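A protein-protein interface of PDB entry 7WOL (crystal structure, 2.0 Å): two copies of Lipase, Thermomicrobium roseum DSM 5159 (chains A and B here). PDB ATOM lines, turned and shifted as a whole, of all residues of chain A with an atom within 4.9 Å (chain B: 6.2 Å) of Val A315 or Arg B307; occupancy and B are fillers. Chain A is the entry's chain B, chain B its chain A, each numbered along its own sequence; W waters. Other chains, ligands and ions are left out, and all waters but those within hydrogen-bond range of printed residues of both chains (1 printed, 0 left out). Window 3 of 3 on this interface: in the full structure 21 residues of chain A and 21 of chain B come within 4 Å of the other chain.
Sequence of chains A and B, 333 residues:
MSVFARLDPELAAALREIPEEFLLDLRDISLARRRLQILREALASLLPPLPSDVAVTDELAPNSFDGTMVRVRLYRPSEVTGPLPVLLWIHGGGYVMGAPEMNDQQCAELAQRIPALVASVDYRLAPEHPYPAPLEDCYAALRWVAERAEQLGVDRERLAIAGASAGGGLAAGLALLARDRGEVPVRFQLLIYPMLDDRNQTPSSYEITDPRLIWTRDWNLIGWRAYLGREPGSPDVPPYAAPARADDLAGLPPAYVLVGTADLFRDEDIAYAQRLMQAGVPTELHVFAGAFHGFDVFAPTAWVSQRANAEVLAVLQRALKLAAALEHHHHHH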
ATOM      1  N   PHE A 188       0.770  31.025 -25.874  1.00  0.00           N
ATOM      2  CA  PHE A 188      -0.666  31.341 -25.658  1.00  0.00           C
ATOM      3  C   PHE A 188      -0.825  32.236 -24.445  1.00  0.00           C
ATOM      4  O   PHE A 188      -0.018  32.096 -23.523  1.00  0.00           O
ATOM      5  CB  PHE A 188      -1.445  30.033 -25.453  1.00  0.00           C
ATOM      6  CG  PHE A 188      -2.934  30.145 -25.627  1.00  0.00           C
ATOM      7  CD1 PHE A 188      -3.474  30.413 -26.871  1.00  0.00           C
ATOM      8  CD2 PHE A 188      -3.788  29.996 -24.553  1.00  0.00           C
ATOM      9  CE1 PHE A 188      -4.848  30.527 -27.041  1.00  0.00           C
ATOM     10  CE2 PHE A 188      -5.162  30.094 -24.725  1.00  0.00           C
ATOM     11  CZ  PHE A 188      -5.681  30.383 -25.967  1.00  0.00           C
ATOM     12  N   LEU A 190      -4.084  33.276 -21.747  1.00  0.00           N
ATOM     13  CA  LEU A 190      -5.457  32.957 -21.301  1.00  0.00           C
ATOM     14  C   LEU A 190      -5.803  34.020 -20.262  1.00  0.00           C
ATOM     15  O   LEU A 190      -5.201  34.004 -19.179  1.00  0.00           O
ATOM     16  CB  LEU A 190      -5.393  31.529 -20.757  1.00  0.00           C
ATOM     17  CG  LEU A 190      -6.648  30.772 -20.315  1.00  0.00           C
ATOM     18  CD1 LEU A 190      -7.212  31.279 -19.028  1.00  0.00           C
ATOM     19  CD2 LEU A 190      -7.707  30.636 -21.382  1.00  0.00           C
ATOM     20  N   TYR A 256      -7.023  33.949 -25.480  1.00  0.00           N
ATOM     21  CA  TYR A 256      -8.431  33.730 -25.109  1.00  0.00           C
ATOM     22  C   TYR A 256      -8.777  34.752 -24.035  1.00  0.00           C
ATOM     23  O   TYR A 256      -7.987  34.919 -23.091  1.00  0.00           O
ATOM     24  CB  TYR A 256      -8.644  32.294 -24.650  1.00  0.00           C
ATOM     25  CG  TYR A 256     -10.009  31.982 -24.098  1.00  0.00           C
ATOM     26  CD1 TYR A 256     -10.284  32.149 -22.754  1.00  0.00           C
ATOM     27  CD2 TYR A 256     -11.014  31.476 -24.909  1.00  0.00           C
ATOM     28  CE1 TYR A 256     -11.524  31.848 -22.227  1.00  0.00           C
ATOM     29  CE2 TYR A 256     -12.264  31.175 -24.396  1.00  0.00           C
ATOM     30  CZ  TYR A 256     -12.519  31.350 -23.051  1.00  0.00           C
ATOM     31  OH  TYR A 256     -13.745  31.070 -22.501  1.00  0.00           O
ATOM     32  N   GLU A 284      -9.757  34.414 -29.292  1.00  0.00           N
ATOM     33  CA  GLU A 284     -11.128  33.990 -28.964  1.00  0.00           C
ATOM     34  C   GLU A 284     -11.611  34.882 -27.823  1.00  0.00           C
ATOM     35  O   GLU A 284     -10.870  35.059 -26.837  1.00  0.00           O
ATOM     36  CB  GLU A 284     -11.144  32.507 -28.608  1.00  0.00           C
ATOM     37  CG  GLU A 284     -12.476  31.985 -28.151  1.00  0.00           C
ATOM     38  CD  GLU A 284     -12.543  30.464 -28.062  1.00  0.00           C
ATOM     39  OE1 GLU A 284     -13.528  29.971 -27.490  1.00  0.00           O
ATOM     40  OE2 GLU A 284     -11.588  29.772 -28.534  1.00  0.00           O
ATOM     41  N   GLU A 311     -14.810  25.307 -21.086  1.00  0.00           N
ATOM     42  CA  GLU A 311     -14.206  25.960 -22.266  1.00  0.00           C
ATOM     43  C   GLU A 311     -12.740  26.325 -21.973  1.00  0.00           C
ATOM     44  O   GLU A 311     -11.909  26.144 -22.838  1.00  0.00           O
ATOM     45  CB  GLU A 311     -15.023  27.190 -22.640  1.00  0.00           C
ATOM     46  CG  GLU A 311     -14.564  27.794 -23.943  1.00  0.00           C
ATOM     47  CD  GLU A 311     -15.543  28.821 -24.487  1.00  0.00           C
ATOM     48  OE1 GLU A 311     -16.460  28.393 -25.193  1.00  0.00           O
ATOM     49  OE2 GLU A 311     -15.401  30.040 -24.155  1.00  0.00           O
ATOM     50  N   VAL A 312     -12.442  26.891 -20.819  1.00  0.00           N
ATOM     51  CA  VAL A 312     -11.033  27.246 -20.475  1.00  0.00           C
ATOM     52  C   VAL A 312     -10.154  25.980 -20.605  1.00  0.00           C
ATOM     53  O   VAL A 312      -9.084  26.044 -21.249  1.00  0.00           O
ATOM     54  CB  VAL A 312     -10.977  27.872 -19.075  1.00  0.00           C
ATOM     55  CG1 VAL A 312      -9.553  27.901 -18.524  1.00  0.00           C
ATOM     56  CG2 VAL A 312     -11.612  29.262 -19.082  1.00  0.00           C
ATOM     57  N   LEU A 313     -10.616  24.849 -20.074  1.00  0.00           N
ATOM     58  CA  LEU A 313      -9.878  23.558 -20.174  1.00  0.00           C
ATOM     59  C   LEU A 313      -9.702  23.170 -21.646  1.00  0.00           C
ATOM     60  O   LEU A 313      -8.561  22.855 -22.062  1.00  0.00           O
ATOM     61  CB  LEU A 313     -10.634  22.482 -19.383  1.00  0.00           C
ATOM     62  CG  LEU A 313     -10.040  21.076 -19.503  1.00  0.00           C
ATOM     63  CD1 LEU A 313      -8.591  21.062 -19.011  1.00  0.00           C
ATOM     64  CD2 LEU A 313     -10.890  20.063 -18.751  1.00  0.00           C
ATOM     65  N   ALA A 314     -10.768  23.250 -22.449  1.00  0.00           N
ATOM     66  CA  ALA A 314     -10.744  22.795 -23.859  1.00  0.00           C
ATOM     67  C   ALA A 314      -9.773  23.657 -24.671  1.00  0.00           C
ATOM     68  O   ALA A 314      -9.047  23.107 -25.538  1.00  0.00           O
ATOM     69  CB  ALA A 314     -12.133  22.809 -24.453  1.00  0.00           C
ATOM     70  N   VAL A 315      -9.724  24.970 -24.422  1.00  0.00           N
ATOM     71  CA  VAL A 315      -8.852  25.841 -25.259  1.00  0.00           C
ATOM     72  C   VAL A 315      -7.395  25.632 -24.825  1.00  0.00           C
ATOM     73  O   VAL A 315      -6.518  25.713 -25.694  1.00  0.00           O
ATOM     74  CB  VAL A 315      -9.263  27.329 -25.267  1.00  0.00           C
ATOM     75  CG1 VAL A 315     -10.740  27.504 -25.604  1.00  0.00           C
ATOM     76  CG2 VAL A 315      -8.909  28.051 -23.992  1.00  0.00           C
ATOM     77  N   LEU A 316      -7.145  25.409 -23.542  1.00  0.00           N
ATOM     78  CA  LEU A 316      -5.761  25.138 -23.026  1.00  0.00           C
ATOM     79  C   LEU A 316      -5.278  23.775 -23.552  1.00  0.00           C
ATOM     80  O   LEU A 316      -4.130  23.695 -23.974  1.00  0.00           O
ATOM     81  CB  LEU A 316      -5.778  25.173 -21.496  1.00  0.00           C
ATOM     82  CG  LEU A 316      -5.874  26.570 -20.879  1.00  0.00           C
ATOM     83  CD1 LEU A 316      -6.058  26.498 -19.384  1.00  0.00           C
ATOM     84  CD2 LEU A 316      -4.657  27.414 -21.232  1.00  0.00           C
ATOM     85  N   GLN A 317      -6.144  22.755 -23.567  1.00  0.00           N
ATOM     86  CA  GLN A 317      -5.814  21.423 -24.146  1.00  0.00           C
ATOM     87  C   GLN A 317      -5.374  21.589 -25.590  1.00  0.00           C
ATOM     88  O   GLN A 317      -4.298  21.064 -25.957  1.00  0.00           O
ATOM     89  CB  GLN A 317      -7.002  20.476 -24.031  1.00  0.00           C
ATOM     90  CG  GLN A 317      -7.178  19.988 -22.610  1.00  0.00           C
ATOM     91  CD  GLN A 317      -8.461  19.222 -22.428  1.00  0.00           C
ATOM     92  OE1 GLN A 317      -9.446  19.432 -23.135  1.00  0.00           O
ATOM     93  NE2 GLN A 317      -8.469  18.368 -21.422  1.00  0.00           N
ATOM     94  N   ARG A 318      -6.158  22.329 -26.373  1.00  0.00           N
ATOM     95  CA  ARG A 318      -5.902  22.534 -27.819  1.00  0.00           C
ATOM     96  C   ARG A 318      -4.616  23.342 -28.009  1.00  0.00           C
ATOM     97  O   ARG A 318      -3.818  22.988 -28.904  1.00  0.00           O
ATOM     98  CB  ARG A 318      -7.097  23.232 -28.466  1.00  0.00           C
ATOM     99  CG  ARG A 318      -6.970  23.394 -29.969  1.00  0.00           C
ATOM    100  CD  ARG A 318      -7.259  22.058 -30.629  1.00  0.00           C
ATOM    101  NE  ARG A 318      -7.341  22.177 -32.073  1.00  0.00           N
ATOM    102  CZ  ARG A 318      -7.661  21.174 -32.892  1.00  0.00           C
ATOM    103  NH1 ARG A 318      -7.928  19.968 -32.411  1.00  0.00           N
ATOM    104  NH2 ARG A 318      -7.718  21.388 -34.193  1.00  0.00           N
ATOM    105  N   ALA A 319      -4.430  24.421 -27.244  1.00  0.00           N
ATOM    106  CA  ALA A 319      -3.274  25.332 -27.420  1.00  0.00           C
ATOM    107  C   ALA A 319      -1.968  24.614 -27.040  1.00  0.00           C
ATOM    108  O   ALA A 319      -0.948  24.958 -27.614  1.00  0.00           O
ATOM    109  CB  ALA A 319      -3.446  26.581 -26.592  1.00  0.00           C
ATOM    110  N   HIS B 286     -19.615  35.311 -28.643  1.00  0.00           N
ATOM    111  CA  HIS B 286     -18.501  34.352 -28.827  1.00  0.00           C
ATOM    112  C   HIS B 286     -17.830  34.631 -30.163  1.00  0.00           C
ATOM    113  O   HIS B 286     -18.484  34.460 -31.240  1.00  0.00           O
ATOM    114  CB  HIS B 286     -18.988  32.913 -28.656  1.00  0.00           C
ATOM    115  CG  HIS B 286     -17.888  31.978 -28.276  1.00  0.00           C
ATOM    116  ND1 HIS B 286     -18.132  30.706 -27.770  1.00  0.00           N
ATOM    117  CD2 HIS B 286     -16.537  32.133 -28.296  1.00  0.00           C
ATOM    118  CE1 HIS B 286     -16.973  30.130 -27.480  1.00  0.00           C
ATOM    119  NE2 HIS B 286     -15.974  30.982 -27.815  1.00  0.00           N
ATOM    120  N   PHE B 288     -14.800  33.424 -32.478  1.00  0.00           N
ATOM    121  CA  PHE B 288     -13.958  32.216 -32.682  1.00  0.00           C
ATOM    122  C   PHE B 288     -12.701  32.593 -33.466  1.00  0.00           C
ATOM    123  O   PHE B 288     -12.796  33.238 -34.508  1.00  0.00           O
ATOM    124  CB  PHE B 288     -14.742  31.099 -33.380  1.00  0.00           C
ATOM    125  CG  PHE B 288     -15.770  30.466 -32.486  1.00  0.00           C
ATOM    126  CD1 PHE B 288     -15.425  29.445 -31.619  1.00  0.00           C
ATOM    127  CD2 PHE B 288     -17.064  30.956 -32.440  1.00  0.00           C
ATOM    128  CE1 PHE B 288     -16.362  28.906 -30.756  1.00  0.00           C
ATOM    129  CE2 PHE B 288     -17.997  30.408 -31.574  1.00  0.00           C
ATOM    130  CZ  PHE B 288     -17.650  29.369 -30.749  1.00  0.00           C
ATOM    131  N   ALA B 302     -14.311  20.404 -38.328  1.00  0.00           N
ATOM    132  CA  ALA B 302     -13.222  21.128 -37.623  1.00  0.00           C
ATOM    133  C   ALA B 302     -13.565  21.259 -36.136  1.00  0.00           C
ATOM    134  O   ALA B 302     -14.746  21.348 -35.791  1.00  0.00           O
ATOM    135  CB  ALA B 302     -12.953  22.461 -38.274  1.00  0.00           C
ATOM    136  N   TRP B 303     -12.551  21.198 -35.271  1.00  0.00           N
ATOM    137  CA  TRP B 303     -12.681  21.326 -33.798  1.00  0.00           C
ATOM    138  C   TRP B 303     -13.478  22.593 -33.443  1.00  0.00           C
ATOM    139  O   TRP B 303     -14.411  22.515 -32.626  1.00  0.00           O
ATOM    140  CB  TRP B 303     -11.278  21.343 -33.196  1.00  0.00           C
ATOM    141  CG  TRP B 303     -11.190  21.622 -31.730  1.00  0.00           C
ATOM    142  CD1 TRP B 303     -11.357  20.730 -30.709  1.00  0.00           C
ATOM    143  CD2 TRP B 303     -10.854  22.881 -31.120  1.00  0.00           C
ATOM    144  NE1 TRP B 303     -11.172  21.358 -29.508  1.00  0.00           N
ATOM    145  CE2 TRP B 303     -10.844  22.670 -29.727  1.00  0.00           C
ATOM    146  CE3 TRP B 303     -10.536  24.151 -31.614  1.00  0.00           C
ATOM    147  CZ2 TRP B 303     -10.550  23.690 -28.823  1.00  0.00           C
ATOM    148  CZ3 TRP B 303     -10.247  25.163 -30.721  1.00  0.00           C
ATOM    149  CH2 TRP B 303     -10.255  24.930 -29.346  1.00  0.00           C
ATOM    150  N   VAL B 304     -13.139  23.715 -34.058  1.00  0.00           N
ATOM    151  CA  VAL B 304     -13.759  25.034 -33.732  1.00  0.00           C
ATOM    152  C   VAL B 304     -15.221  25.021 -34.213  1.00  0.00           C
ATOM    153  O   VAL B 304     -16.088  25.591 -33.509  1.00  0.00           O
ATOM    154  CB  VAL B 304     -12.930  26.195 -34.305  1.00  0.00           C
ATOM    155  CG1 VAL B 304     -12.997  26.276 -35.822  1.00  0.00           C
ATOM    156  CG2 VAL B 304     -13.324  27.524 -33.671  1.00  0.00           C
ATOM    157  N   SER B 305     -15.506  24.356 -35.338  1.00  0.00           N
ATOM    158  CA  SER B 305     -16.879  24.262 -35.901  1.00  0.00           C
ATOM    159  C   SER B 305     -17.749  23.442 -34.963  1.00  0.00           C
ATOM    160  O   SER B 305     -18.906  23.852 -34.694  1.00  0.00           O
ATOM    161  CB  SER B 305     -16.882  23.705 -37.279  1.00  0.00           C
ATOM    162  OG  SER B 305     -16.138  24.543 -38.139  1.00  0.00           O
ATOM    163  N   GLN B 306     -17.207  22.337 -34.458  1.00  0.00           N
ATOM    164  CA  GLN B 306     -17.928  21.461 -33.516  1.00  0.00           C
ATOM    165  C   GLN B 306     -18.256  22.255 -32.256  1.00  0.00           C
ATOM    166  O   GLN B 306     -19.374  22.098 -31.725  1.00  0.00           O
ATOM    167  CB  GLN B 306     -17.102  20.206 -33.218  1.00  0.00           C
ATOM    168  CG  GLN B 306     -17.021  19.247 -34.403  1.00  0.00           C
ATOM    169  CD  GLN B 306     -16.163  18.047 -34.084  1.00  0.00           C
ATOM    170  OE1 GLN B 306     -15.257  17.692 -34.826  1.00  0.00           O
ATOM    171  NE2 GLN B 306     -16.416  17.433 -32.951  1.00  0.00           N
ATOM    172  N   ARG B 307     -17.305  23.036 -31.733  1.00  0.00           N
ATOM    173  CA  ARG B 307     -17.557  23.833 -30.504  1.00  0.00           C
ATOM    174  C   ARG B 307     -18.696  24.832 -30.796  1.00  0.00           C
ATOM    175  O   ARG B 307     -19.604  24.965 -29.940  1.00  0.00           O
ATOM    176  CB  ARG B 307     -16.280  24.527 -30.020  1.00  0.00           C
ATOM    177  CG  ARG B 307     -15.164  23.599 -29.560  1.00  0.00           C
ATOM    178  CD  ARG B 307     -13.873  24.349 -29.223  1.00  0.00           C
ATOM    179  NE  ARG B 307     -14.177  25.409 -28.283  1.00  0.00           N
ATOM    180  CZ  ARG B 307     -13.682  26.651 -28.296  1.00  0.00           C
ATOM    181  NH1 ARG B 307     -12.773  27.043 -29.177  1.00  0.00           N
ATOM    182  NH2 ARG B 307     -14.116  27.496 -27.390  1.00  0.00           N
ATOM    183  N   ALA B 308     -18.641  25.519 -31.937  1.00  0.00           N
ATOM    184  CA  ALA B 308     -19.649  26.524 -32.345  1.00  0.00           C
ATOM    185  C   ALA B 308     -21.026  25.841 -32.424  1.00  0.00           C
ATOM    186  O   ALA B 308     -21.984  26.321 -31.763  1.00  0.00           O
ATOM    187  CB  ALA B 308     -19.226  27.169 -33.633  1.00  0.00           C
ATOM    188  N   ASN B 309     -21.111  24.685 -33.105  1.00  0.00           N
ATOM    189  CA  ASN B 309     -22.405  23.981 -33.330  1.00  0.00           C
ATOM    190  C   ASN B 309     -22.941  23.462 -32.005  1.00  0.00           C
ATOM    191  O   ASN B 309     -24.167  23.578 -31.763  1.00  0.00           O
ATOM    192  CB  ASN B 309     -22.287  22.896 -34.408  1.00  0.00           C
ATOM    193  CG  ASN B 309     -22.125  23.520 -35.774  1.00  0.00           C
ATOM    194  OD1 ASN B 309     -22.708  24.570 -36.047  1.00  0.00           O
ATOM    195  ND2 ASN B 309     -21.313  22.916 -36.629  1.00  0.00           N
ATOM    196  N   ALA B 310     -22.078  22.930 -31.141  1.00  0.00           N
ATOM    197  CA  ALA B 310     -22.500  22.425 -29.814  1.00  0.00           C
ATOM    198  C   ALA B 310     -23.010  23.593 -28.959  1.00  0.00           C
ATOM    199  O   ALA B 310     -23.953  23.405 -28.166  1.00  0.00           O
ATOM    200  CB  ALA B 310     -21.377  21.688 -29.115  1.00  0.00           C
ATOM    201  N   GLU B 311     -22.402  24.768 -29.081  1.00  0.00           N
ATOM    202  CA  GLU B 311     -22.796  25.921 -28.229  1.00  0.00           C
ATOM    203  C   GLU B 311     -24.142  26.498 -28.707  1.00  0.00           C
ATOM    204  O   GLU B 311     -24.981  26.834 -27.852  1.00  0.00           O
ATOM    205  CB  GLU B 311     -21.690  26.976 -28.224  1.00  0.00           C
ATOM    206  CG  GLU B 311     -22.038  28.168 -27.370  1.00  0.00           C
ATOM    207  CD  GLU B 311     -20.811  29.029 -27.139  1.00  0.00           C
ATOM    208  OE1 GLU B 311     -20.032  28.654 -26.242  1.00  0.00           O
ATOM    209  OE2 GLU B 311     -20.601  29.993 -27.926  1.00  0.00           O
ATOM    210  N   VAL B 312     -24.343  26.635 -30.017  1.00  0.00           N
ATOM    211  CA  VAL B 312     -25.647  27.115 -30.558  1.00  0.00           C
ATOM    212  C   VAL B 312     -26.766  26.228 -29.998  1.00  0.00           C
ATOM    213  O   VAL B 312     -27.750  26.790 -29.513  1.00  0.00           O
ATOM    214  CB  VAL B 312     -25.647  27.160 -32.089  1.00  0.00           C
ATOM    215  CG1 VAL B 312     -27.052  27.318 -32.678  1.00  0.00           C
ATOM    216  CG2 VAL B 312     -24.708  28.248 -32.586  1.00  0.00           C
HETATM  217  O   HOH W   1      -9.742  20.836 -26.636  1.00  0.00           O
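Leu A190 touches none of the printed residues of chain B. Of the printed residues of chain B, Glu A311 touches His B286 (2.9 Å), Arg B307 (3.3 Å) and Glu B311 (3.7 Å). Printed residues of chain B within 4 Å of Ala A314: Trp B303. Val A315 touches one residue of chain B. Ser B305 touches none of the printed residues of chain A. Of chain A, only Glu A284, Glu A311 and Val A315 come within 4 Å of Arg B307. The nearest printed residue of chain A that does not touch Arg B307 is Ala A314 (5.1 Å). The nearest printed residue of chain A that does not touch His B286 is Tyr A256 (5.0 Å).
The side-chain carboxylate (OE2) of Glu A311 is in hydrogen-bond range of the side-chain hydroxyl (OH) of Tyr A256, at 2.6 Å. A ring nitrogen (ND1) of His B286 lies within hydrogen-bond range of the side-chain carboxylate (OE2) of Glu B311 (2.6 Å).
The side-chain carboxylate (OE1) of Glu A284 is in hydrogen-bond range of a ring nitrogen (NE2) of His B286 (2.7 Å). The guanidinium group (NH2) of Arg B307 is in salt-bridge range of the side-chain carboxylate (OE1) of Glu A311 (3.3 Å). The guanidinium group (NH2) of Arg B307 lies within salt-bridge range of the side-chain carboxylate (OE1) of Glu A284 (2.5 Å).
Glu A311 touches His B286 (OE1 to CE1, 2.9 Å). Glu B311 touches Glu A311 (OE1 to OE1, 3.7 Å). Ala A314 touches Trp B303. Val A315 touches Arg B307 (CG1 to NH2, 3.8 Å). Trp B303 touches Arg A318.
Glu A311 touches its own counterpart, Glu B311. Of the 8 pairs that touch across the chains among the printed residues, 1 has its exchanged pair printed and touching as well.
Water W1 lies within hydrogen-bond range of the backbone carbonyl oxygen of Ala A314 (2.6 Å) and the indole nitrogen of Trp B303 (3.3 Å).
Hydrophobic or aromatic side chains of chain B within 4 Å of the printed part of chain A: His B286 and Trp B303. Of the 13 printed residues of chain A, 5 touch a printed residue of chain B. Printed residues of chain A that touch a printed residue of chain B: Glu A284, Glu A311, Ala A314, Val A315 and Arg A318. Hydrophobic or aromatic side chains of chain A within 4 Å of the printed part of chain B: Val A315. Among the printed residues, Asp or Glu carboxylates within 4 Å of a Lys or Arg side-chain nitrogen of the other chain: Glu A284 with Arg B307 and Glu A311 with Arg B307.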
